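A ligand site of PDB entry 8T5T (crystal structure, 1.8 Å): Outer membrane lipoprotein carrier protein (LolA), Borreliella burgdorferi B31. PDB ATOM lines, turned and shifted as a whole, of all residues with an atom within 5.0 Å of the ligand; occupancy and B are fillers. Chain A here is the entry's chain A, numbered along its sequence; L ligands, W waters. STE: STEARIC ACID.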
ATOM      1  N   MET A  22      29.688   4.821 -17.850  1.00  0.00           N
ATOM      2  CA  MET A  22      30.692   3.885 -17.391  1.00  0.00           C
ATOM      3  C   MET A  22      30.131   2.471 -17.387  1.00  0.00           C
ATOM      4  O   MET A  22      29.017   2.249 -16.906  1.00  0.00           O
ATOM      5  CB  MET A  22      31.126   4.153 -15.957  1.00  0.00           C
ATOM      6  CG  MET A  22      32.352   3.407 -15.515  1.00  0.00           C
ATOM      7  SD  MET A  22      32.818   3.977 -13.877  1.00  0.00           S
ATOM      8  CE  MET A  22      31.548   3.282 -12.881  1.00  0.00           C
ATOM      9  N   ILE A  26      31.550  -5.639 -11.593  1.00  0.00           N
ATOM     10  CA  ILE A  26      31.305  -5.187 -10.240  1.00  0.00           C
ATOM     11  C   ILE A  26      31.168  -6.404  -9.333  1.00  0.00           C
ATOM     12  O   ILE A  26      30.491  -7.382  -9.693  1.00  0.00           O
ATOM     13  CB  ILE A  26      30.077  -4.257 -10.151  1.00  0.00           C
ATOM     14  CG1 ILE A  26      29.876  -3.784  -8.712  1.00  0.00           C
ATOM     15  CG2 ILE A  26      28.789  -4.916 -10.665  1.00  0.00           C
ATOM     16  CD1 ILE A  26      28.836  -2.654  -8.540  1.00  0.00           C
ATOM     17  N   PHE A  28      30.232  -6.909  -5.171  1.00  0.00           N
ATOM     18  CA  PHE A  28      29.829  -6.155  -3.996  1.00  0.00           C
ATOM     19  C   PHE A  28      29.232  -7.109  -2.980  1.00  0.00           C
ATOM     20  O   PHE A  28      28.678  -8.143  -3.347  1.00  0.00           O
ATOM     21  CB  PHE A  28      28.840  -5.039  -4.341  1.00  0.00           C
ATOM     22  CG  PHE A  28      27.536  -5.475  -4.981  1.00  0.00           C
ATOM     23  CD1 PHE A  28      27.461  -5.681  -6.346  1.00  0.00           C
ATOM     24  CD2 PHE A  28      26.369  -5.550  -4.239  1.00  0.00           C
ATOM     25  CE1 PHE A  28      26.301  -6.007  -6.948  1.00  0.00           C
ATOM     26  CE2 PHE A  28      25.181  -5.865  -4.863  1.00  0.00           C
ATOM     27  CZ  PHE A  28      25.148  -6.083  -6.205  1.00  0.00           C
ATOM     28  N   LEU A  30      26.564  -7.674   0.099  1.00  0.00           N
ATOM     29  CA  LEU A  30      25.371  -7.228   0.795  1.00  0.00           C
ATOM     30  C   LEU A  30      24.820  -8.410   1.575  1.00  0.00           C
ATOM     31  O   LEU A  30      24.804  -9.539   1.068  1.00  0.00           O
ATOM     32  CB  LEU A  30      24.300  -6.693  -0.171  1.00  0.00           C
ATOM     33  CG  LEU A  30      24.503  -5.245  -0.594  1.00  0.00           C
ATOM     34  CD1 LEU A  30      23.548  -4.865  -1.706  1.00  0.00           C
ATOM     35  CD2 LEU A  30      24.312  -4.335   0.573  1.00  0.00           C
ATOM     36  N   LEU A  39      28.047  -3.493 -14.070  1.00  0.00           N
ATOM     37  CA  LEU A  39      27.489  -2.189 -13.770  1.00  0.00           C
ATOM     38  C   LEU A  39      27.477  -1.321 -15.031  1.00  0.00           C
ATOM     39  O   LEU A  39      28.508  -1.166 -15.689  1.00  0.00           O
ATOM     40  CB  LEU A  39      28.315  -1.508 -12.682  1.00  0.00           C
ATOM     41  CG  LEU A  39      28.084  -0.037 -12.416  1.00  0.00           C
ATOM     42  CD1 LEU A  39      26.751   0.182 -11.703  1.00  0.00           C
ATOM     43  CD2 LEU A  39      29.192   0.527 -11.570  1.00  0.00           C
ATOM     44  N   TYR A  41      26.610   2.644 -15.629  1.00  0.00           N
ATOM     45  CA  TYR A  41      26.331   3.907 -14.927  1.00  0.00           C
ATOM     46  C   TYR A  41      26.145   4.992 -15.976  1.00  0.00           C
ATOM     47  O   TYR A  41      27.056   5.233 -16.782  1.00  0.00           O
ATOM     48  CB  TYR A  41      27.465   4.284 -13.955  1.00  0.00           C
ATOM     49  CG  TYR A  41      27.020   5.204 -12.827  1.00  0.00           C
ATOM     50  CD1 TYR A  41      26.768   6.563 -13.059  1.00  0.00           C
ATOM     51  CD2 TYR A  41      26.916   4.724 -11.510  1.00  0.00           C
ATOM     52  CE1 TYR A  41      26.372   7.394 -12.021  1.00  0.00           C
ATOM     53  CE2 TYR A  41      26.520   5.553 -10.482  1.00  0.00           C
ATOM     54  CZ  TYR A  41      26.244   6.884 -10.737  1.00  0.00           C
ATOM     55  OH  TYR A  41      25.847   7.699  -9.705  1.00  0.00           O
ATOM     56  N   ASP A  45      23.702  10.183 -12.525  1.00  0.00           N
ATOM     57  CA  ASP A  45      23.053   9.636 -11.345  1.00  0.00           C
ATOM     58  C   ASP A  45      22.190   8.396 -11.573  1.00  0.00           C
ATOM     59  O   ASP A  45      21.385   8.080 -10.685  1.00  0.00           O
ATOM     60  CB  ASP A  45      22.127  10.718 -10.671  1.00  0.00           C
ATOM     61  CG  ASP A  45      21.058  11.275 -11.613  1.00  0.00           C
ATOM     62  OD1 ASP A  45      21.028  10.932 -12.825  1.00  0.00           O
ATOM     63  OD2 ASP A  45      20.255  12.123 -11.145  1.00  0.00           O
ATOM     64  N   PHE A  47      21.923   4.111 -12.640  1.00  0.00           N
ATOM     65  CA  PHE A  47      22.681   2.909 -12.963  1.00  0.00           C
ATOM     66  C   PHE A  47      21.809   1.664 -12.930  1.00  0.00           C
ATOM     67  O   PHE A  47      20.711   1.641 -12.370  1.00  0.00           O
ATOM     68  CB  PHE A  47      23.920   2.754 -12.037  1.00  0.00           C
ATOM     69  CG  PHE A  47      23.617   2.453 -10.570  1.00  0.00           C
ATOM     70  CD1 PHE A  47      23.253   1.197 -10.168  1.00  0.00           C
ATOM     71  CD2 PHE A  47      23.836   3.410  -9.601  1.00  0.00           C
ATOM     72  CE1 PHE A  47      23.017   0.916  -8.843  1.00  0.00           C
ATOM     73  CE2 PHE A  47      23.613   3.122  -8.244  1.00  0.00           C
ATOM     74  CZ  PHE A  47      23.199   1.864  -7.892  1.00  0.00           C
ATOM     75  N   ILE A  49      22.605  -2.715 -12.533  1.00  0.00           N
ATOM     76  CA  ILE A  49      23.531  -3.836 -12.352  1.00  0.00           C
ATOM     77  C   ILE A  49      22.800  -5.113 -12.739  1.00  0.00           C
ATOM     78  O   ILE A  49      21.755  -5.436 -12.156  1.00  0.00           O
ATOM     79  CB  ILE A  49      24.046  -3.957 -10.911  1.00  0.00           C
ATOM     80  CG1 ILE A  49      24.839  -2.706 -10.466  1.00  0.00           C
ATOM     81  CG2 ILE A  49      24.970  -5.186 -10.772  1.00  0.00           C
ATOM     82  CD1 ILE A  49      25.074  -2.604  -9.001  1.00  0.00           C
ATOM     83  N   GLY A  62      19.167   7.482  -8.677  1.00  0.00           N
ATOM     84  CA  GLY A  62      19.827   8.447  -7.804  1.00  0.00           C
ATOM     85  C   GLY A  62      19.085   8.730  -6.517  1.00  0.00           C
ATOM     86  O   GLY A  62      19.669   9.304  -5.591  1.00  0.00           O
ATOM     87  N   LEU A  65      16.796   2.767  -4.935  1.00  0.00           N
ATOM     88  CA  LEU A  65      17.425   1.538  -5.394  1.00  0.00           C
ATOM     89  C   LEU A  65      16.348   0.467  -5.459  1.00  0.00           C
ATOM     90  O   LEU A  65      15.755   0.148  -4.418  1.00  0.00           O
ATOM     91  CB  LEU A  65      18.544   1.147  -4.449  1.00  0.00           C
ATOM     92  CG  LEU A  65      19.392  -0.080  -4.809  1.00  0.00           C
ATOM     93  CD1 LEU A  65      20.042   0.062  -6.133  1.00  0.00           C
ATOM     94  CD2 LEU A  65      20.452  -0.242  -3.679  1.00  0.00           C
ATOM     95  N   LEU A  80      18.094   4.934  -1.902  1.00  0.00           N
ATOM     96  CA  LEU A  80      19.509   4.700  -2.185  1.00  0.00           C
ATOM     97  C   LEU A  80      20.385   5.217  -1.061  1.00  0.00           C
ATOM     98  O   LEU A  80      21.363   4.558  -0.650  1.00  0.00           O
ATOM     99  CB  LEU A  80      19.858   5.397  -3.497  1.00  0.00           C
ATOM    100  CG  LEU A  80      21.317   5.249  -3.951  1.00  0.00           C
ATOM    101  CD1 LEU A  80      21.650   3.804  -4.248  1.00  0.00           C
ATOM    102  CD2 LEU A  80      21.631   6.123  -5.147  1.00  0.00           C
ATOM    103  N   LEU A  81      20.010   6.351  -0.475  1.00  0.00           N
ATOM    104  CA  LEU A  81      20.830   6.964   0.581  1.00  0.00           C
ATOM    105  C   LEU A  81      19.945   7.951   1.323  1.00  0.00           C
ATOM    106  O   LEU A  81      19.985   9.160   1.097  1.00  0.00           O
ATOM    107  CB  LEU A  81      22.075   7.634  -0.023  1.00  0.00           C
ATOM    108  CG  LEU A  81      23.118   8.187   0.942  1.00  0.00           C
ATOM    109  CD1 LEU A  81      23.664   7.152   1.866  1.00  0.00           C
ATOM    110  CD2 LEU A  81      24.278   8.841   0.158  1.00  0.00           C
ATOM    111  N   GLY A  88      23.590  11.818  -7.801  1.00  0.00           N
ATOM    112  CA  GLY A  88      24.640  10.947  -8.298  1.00  0.00           C
ATOM    113  C   GLY A  88      25.833  10.929  -7.369  1.00  0.00           C
ATOM    114  O   GLY A  88      25.985  11.766  -6.479  1.00  0.00           O
ATOM    115  N   LEU A  89      26.695   9.946  -7.570  1.00  0.00           N
ATOM    116  CA  LEU A  89      27.754   9.692  -6.581  1.00  0.00           C
ATOM    117  C   LEU A  89      28.658  10.901  -6.396  1.00  0.00           C
ATOM    118  O   LEU A  89      28.991  11.297  -5.268  1.00  0.00           O
ATOM    119  CB  LEU A  89      28.575   8.477  -7.006  1.00  0.00           C
ATOM    120  CG  LEU A  89      29.841   8.217  -6.205  1.00  0.00           C
ATOM    121  CD1 LEU A  89      29.448   7.680  -4.866  1.00  0.00           C
ATOM    122  CD2 LEU A  89      30.726   7.229  -6.999  1.00  0.00           C
ATOM    123  N   VAL A  92      27.063  13.863  -4.587  1.00  0.00           N
ATOM    124  CA  VAL A  92      26.864  13.530  -3.175  1.00  0.00           C
ATOM    125  C   VAL A  92      28.175  13.634  -2.429  1.00  0.00           C
ATOM    126  O   VAL A  92      28.262  14.304  -1.396  1.00  0.00           O
ATOM    127  CB  VAL A  92      26.220  12.141  -3.063  1.00  0.00           C
ATOM    128  CG1 VAL A  92      26.329  11.579  -1.632  1.00  0.00           C
ATOM    129  CG2 VAL A  92      24.741  12.239  -3.520  1.00  0.00           C
ATOM    130  N   PHE A 137      32.569   6.962   3.349  1.00  0.00           N
ATOM    131  CA  PHE A 137      33.062   6.106   2.254  1.00  0.00           C
ATOM    132  C   PHE A 137      34.589   6.200   2.218  1.00  0.00           C
ATOM    133  O   PHE A 137      35.182   7.261   2.462  1.00  0.00           O
ATOM    134  CB  PHE A 137      32.557   6.509   0.825  1.00  0.00           C
ATOM    135  CG  PHE A 137      31.071   6.558   0.653  1.00  0.00           C
ATOM    136  CD1 PHE A 137      30.363   7.674   1.000  1.00  0.00           C
ATOM    137  CD2 PHE A 137      30.380   5.484   0.082  1.00  0.00           C
ATOM    138  CE1 PHE A 137      28.987   7.755   0.796  1.00  0.00           C
ATOM    139  CE2 PHE A 137      29.015   5.534  -0.125  1.00  0.00           C
ATOM    140  CZ  PHE A 137      28.294   6.667   0.228  1.00  0.00           C
ATOM    141  N   ILE A 147      37.947   4.564 -10.535  1.00  0.00           N
ATOM    142  CA  ILE A 147      37.596   4.013  -9.234  1.00  0.00           C
ATOM    143  C   ILE A 147      37.909   2.527  -9.217  1.00  0.00           C
ATOM    144  O   ILE A 147      37.459   1.772 -10.093  1.00  0.00           O
ATOM    145  CB  ILE A 147      36.111   4.258  -8.932  1.00  0.00           C
ATOM    146  CG1 ILE A 147      35.812   5.756  -8.901  1.00  0.00           C
ATOM    147  CG2 ILE A 147      35.703   3.634  -7.567  1.00  0.00           C
ATOM    148  CD1 ILE A 147      34.317   6.105  -9.087  1.00  0.00           C
ATOM    149  N   ILE A 150      35.090   1.074  -3.671  1.00  0.00           N
ATOM    150  CA  ILE A 150      34.316   1.944  -2.814  1.00  0.00           C
ATOM    151  C   ILE A 150      33.933   1.109  -1.607  1.00  0.00           C
ATOM    152  O   ILE A 150      33.305   0.052  -1.768  1.00  0.00           O
ATOM    153  CB  ILE A 150      33.037   2.473  -3.483  1.00  0.00           C
ATOM    154  CG1 ILE A 150      33.369   3.306  -4.688  1.00  0.00           C
ATOM    155  CG2 ILE A 150      32.183   3.253  -2.505  1.00  0.00           C
ATOM    156  CD1 ILE A 150      32.200   3.356  -5.627  1.00  0.00           C
ATOM    157  N   ALA A 152      31.689   1.369   1.746  1.00  0.00           N
ATOM    158  CA  ALA A 152      30.662   2.171   2.367  1.00  0.00           C
ATOM    159  C   ALA A 152      30.412   1.655   3.771  1.00  0.00           C
ATOM    160  O   ALA A 152      30.236   0.428   3.972  1.00  0.00           O
ATOM    161  CB  ALA A 152      29.370   2.120   1.553  1.00  0.00           C
ATOM    162  N   ILE A 161      29.977  -2.324   3.274  1.00  0.00           N
ATOM    163  CA  ILE A 161      29.675  -2.705   1.901  1.00  0.00           C
ATOM    164  C   ILE A 161      30.891  -2.381   1.065  1.00  0.00           C
ATOM    165  O   ILE A 161      31.248  -1.202   0.905  1.00  0.00           O
ATOM    166  CB  ILE A 161      28.425  -1.989   1.375  1.00  0.00           C
ATOM    167  CG1 ILE A 161      27.239  -2.282   2.275  1.00  0.00           C
ATOM    168  CG2 ILE A 161      28.179  -2.385  -0.088  1.00  0.00           C
ATOM    169  CD1 ILE A 161      26.061  -1.388   1.977  1.00  0.00           C
ATOM    170  N   ILE A 163      32.623  -2.511  -2.554  1.00  0.00           N
ATOM    171  CA  ILE A 163      32.310  -2.520  -3.972  1.00  0.00           C
ATOM    172  C   ILE A 163      33.622  -2.486  -4.736  1.00  0.00           C
ATOM    173  O   ILE A 163      34.379  -1.511  -4.638  1.00  0.00           O
ATOM    174  CB  ILE A 163      31.434  -1.317  -4.365  1.00  0.00           C
ATOM    175  CG1 ILE A 163      30.152  -1.323  -3.547  1.00  0.00           C
ATOM    176  CG2 ILE A 163      31.148  -1.356  -5.879  1.00  0.00           C
ATOM    177  CD1 ILE A 163      29.496  -0.030  -3.512  1.00  0.00           C
ATOM    178  N   LEU A 165      35.302  -2.470  -8.449  1.00  0.00           N
ATOM    179  CA  LEU A 165      35.100  -2.179  -9.872  1.00  0.00           C
ATOM    180  C   LEU A 165      36.361  -2.581 -10.624  1.00  0.00           C
ATOM    181  O   LEU A 165      37.460  -2.153 -10.249  1.00  0.00           O
ATOM    182  CB  LEU A 165      34.808  -0.696 -10.067  1.00  0.00           C
ATOM    183  CG  LEU A 165      33.594  -0.157  -9.313  1.00  0.00           C
ATOM    184  CD1 LEU A 165      33.346   1.321  -9.715  1.00  0.00           C
ATOM    185  CD2 LEU A 165      32.320  -0.963  -9.566  1.00  0.00           C
ATOM    186  N   TYR A 195      20.974  -2.288   3.441  1.00  0.00           N
ATOM    187  CA  TYR A 195      22.169  -1.877   4.194  1.00  0.00           C
ATOM    188  C   TYR A 195      22.033  -2.214   5.689  1.00  0.00           C
ATOM    189  O   TYR A 195      23.035  -2.498   6.355  1.00  0.00           O
ATOM    190  CB  TYR A 195      22.475  -0.370   4.054  1.00  0.00           C
ATOM    191  CG  TYR A 195      22.320   0.235   2.685  1.00  0.00           C
ATOM    192  CD1 TYR A 195      22.360  -0.532   1.531  1.00  0.00           C
ATOM    193  CD2 TYR A 195      22.125   1.603   2.553  1.00  0.00           C
ATOM    194  CE1 TYR A 195      22.182   0.055   0.272  1.00  0.00           C
ATOM    195  CE2 TYR A 195      21.961   2.190   1.346  1.00  0.00           C
ATOM    196  CZ  TYR A 195      21.994   1.430   0.190  1.00  0.00           C
ATOM    197  OH  TYR A 195      21.811   2.049  -1.037  1.00  0.00           O
HETATM  198  C1  STE L   1      24.659   7.528  -6.352  1.00  0.00           C
HETATM  199  O1  STE L   1      23.730   8.263  -6.744  1.00  0.00           O
HETATM  200  O2  STE L   1      25.316   6.778  -7.137  1.00  0.00           O
HETATM  201  C2  STE L   1      24.984   7.512  -4.813  1.00  0.00           C
HETATM  202  C3  STE L   1      25.787   6.302  -4.312  1.00  0.00           C
HETATM  203  C4  STE L   1      25.341   5.644  -2.999  1.00  0.00           C
HETATM  204  C5  STE L   1      26.081   4.343  -2.679  1.00  0.00           C
HETATM  205  C6  STE L   1      25.268   3.252  -1.973  1.00  0.00           C
HETATM  206  C7  STE L   1      26.079   1.957  -1.760  1.00  0.00           C
HETATM  207  C8  STE L   1      25.274   0.672  -1.592  1.00  0.00           C
HETATM  208  C9  STE L   1      24.680   0.124  -2.889  1.00  0.00           C
HETATM  209  C10 STE L   1      24.982  -1.351  -3.198  1.00  0.00           C
HETATM  210  C11 STE L   1      25.075  -1.599  -4.710  1.00  0.00           C
HETATM  211  C12 STE L   1      26.291  -0.941  -5.362  1.00  0.00           C
HETATM  212  C13 STE L   1      26.033   0.235  -6.300  1.00  0.00           C
HETATM  213  C14 STE L   1      27.118   1.303  -6.318  1.00  0.00           C
HETATM  214  C15 STE L   1      27.595   1.744  -7.684  1.00  0.00           C
HETATM  215  C16 STE L   1      28.251   3.114  -7.708  1.00  0.00           C
HETATM  216  C17 STE L   1      29.599   3.155  -8.412  1.00  0.00           C
HETATM  217  C18 STE L   1      29.889   4.340  -9.333  1.00  0.00           C
HETATM  218  O   HOH W   1      22.449   6.274  -8.528  1.00  0.00           O
HETATM  219  O   HOH W   2      22.439  10.077  -5.744  1.00  0.00           O
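The side-chain hydroxyl (OH) of Tyr 41 sits at hydrogen-bond distance from an oxygen (O2) of the ligand (2.8 Å). An oxygen (O2) of the ligand sits close to the backbone NH (N) of Leu 89 (3.5 Å).
CZ of Phe 47 touches C13 of the ligand, at 3.6 Å. CD2 of Leu 80 touches O1 of the ligand, 3.4 Å away. CA of Gly 88 touches O1 of the ligand, 3.2 Å away. Ile 150 touches the ligand. Ile 163 touches the ligand. Tyr 195 touches the ligand. Within 4 Å of the ligand: Tyr 41, Phe 47, Leu 80, Gly 88, Leu 89, Ile 150, Ile 163 and Tyr 195. Along chain A the residues within 4 Å of the ligand span positions 41 to 195. The nearest printed residue that does not touch the ligand is Ile 49 (4.03 Å).
Water W2 lies within hydrogen-bond range of an oxygen (O1) of the ligand (2.4 Å), the backbone carbonyl oxygen of Gly 62 (2.9 Å) and the backbone NH of Gly 88 (2.9 Å). Water W1 bridges an oxygen (O1) of the ligand (3.0 Å) and the backbone carbonyl oxygen (O) of Asp 45 (3.0 Å).
The side-chain hydroxyl (OH) of Tyr 41 sits at hydrogen-bond distance from the backbone NH (N) of Leu 89 (3.2 Å). N of Tyr 41 lies within hydrogen-bond range of O of Met 22 (2.8 Å). The backbone NH of Ile 163 lies within hydrogen-bond range of the backbone carbonyl oxygen of Ile 150 (2.8 Å). The backbone carbonyl oxygen (O) of Leu 80 sits at hydrogen-bond distance from the side-chain hydroxyl (OH) of Tyr 195 (2.6 Å).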
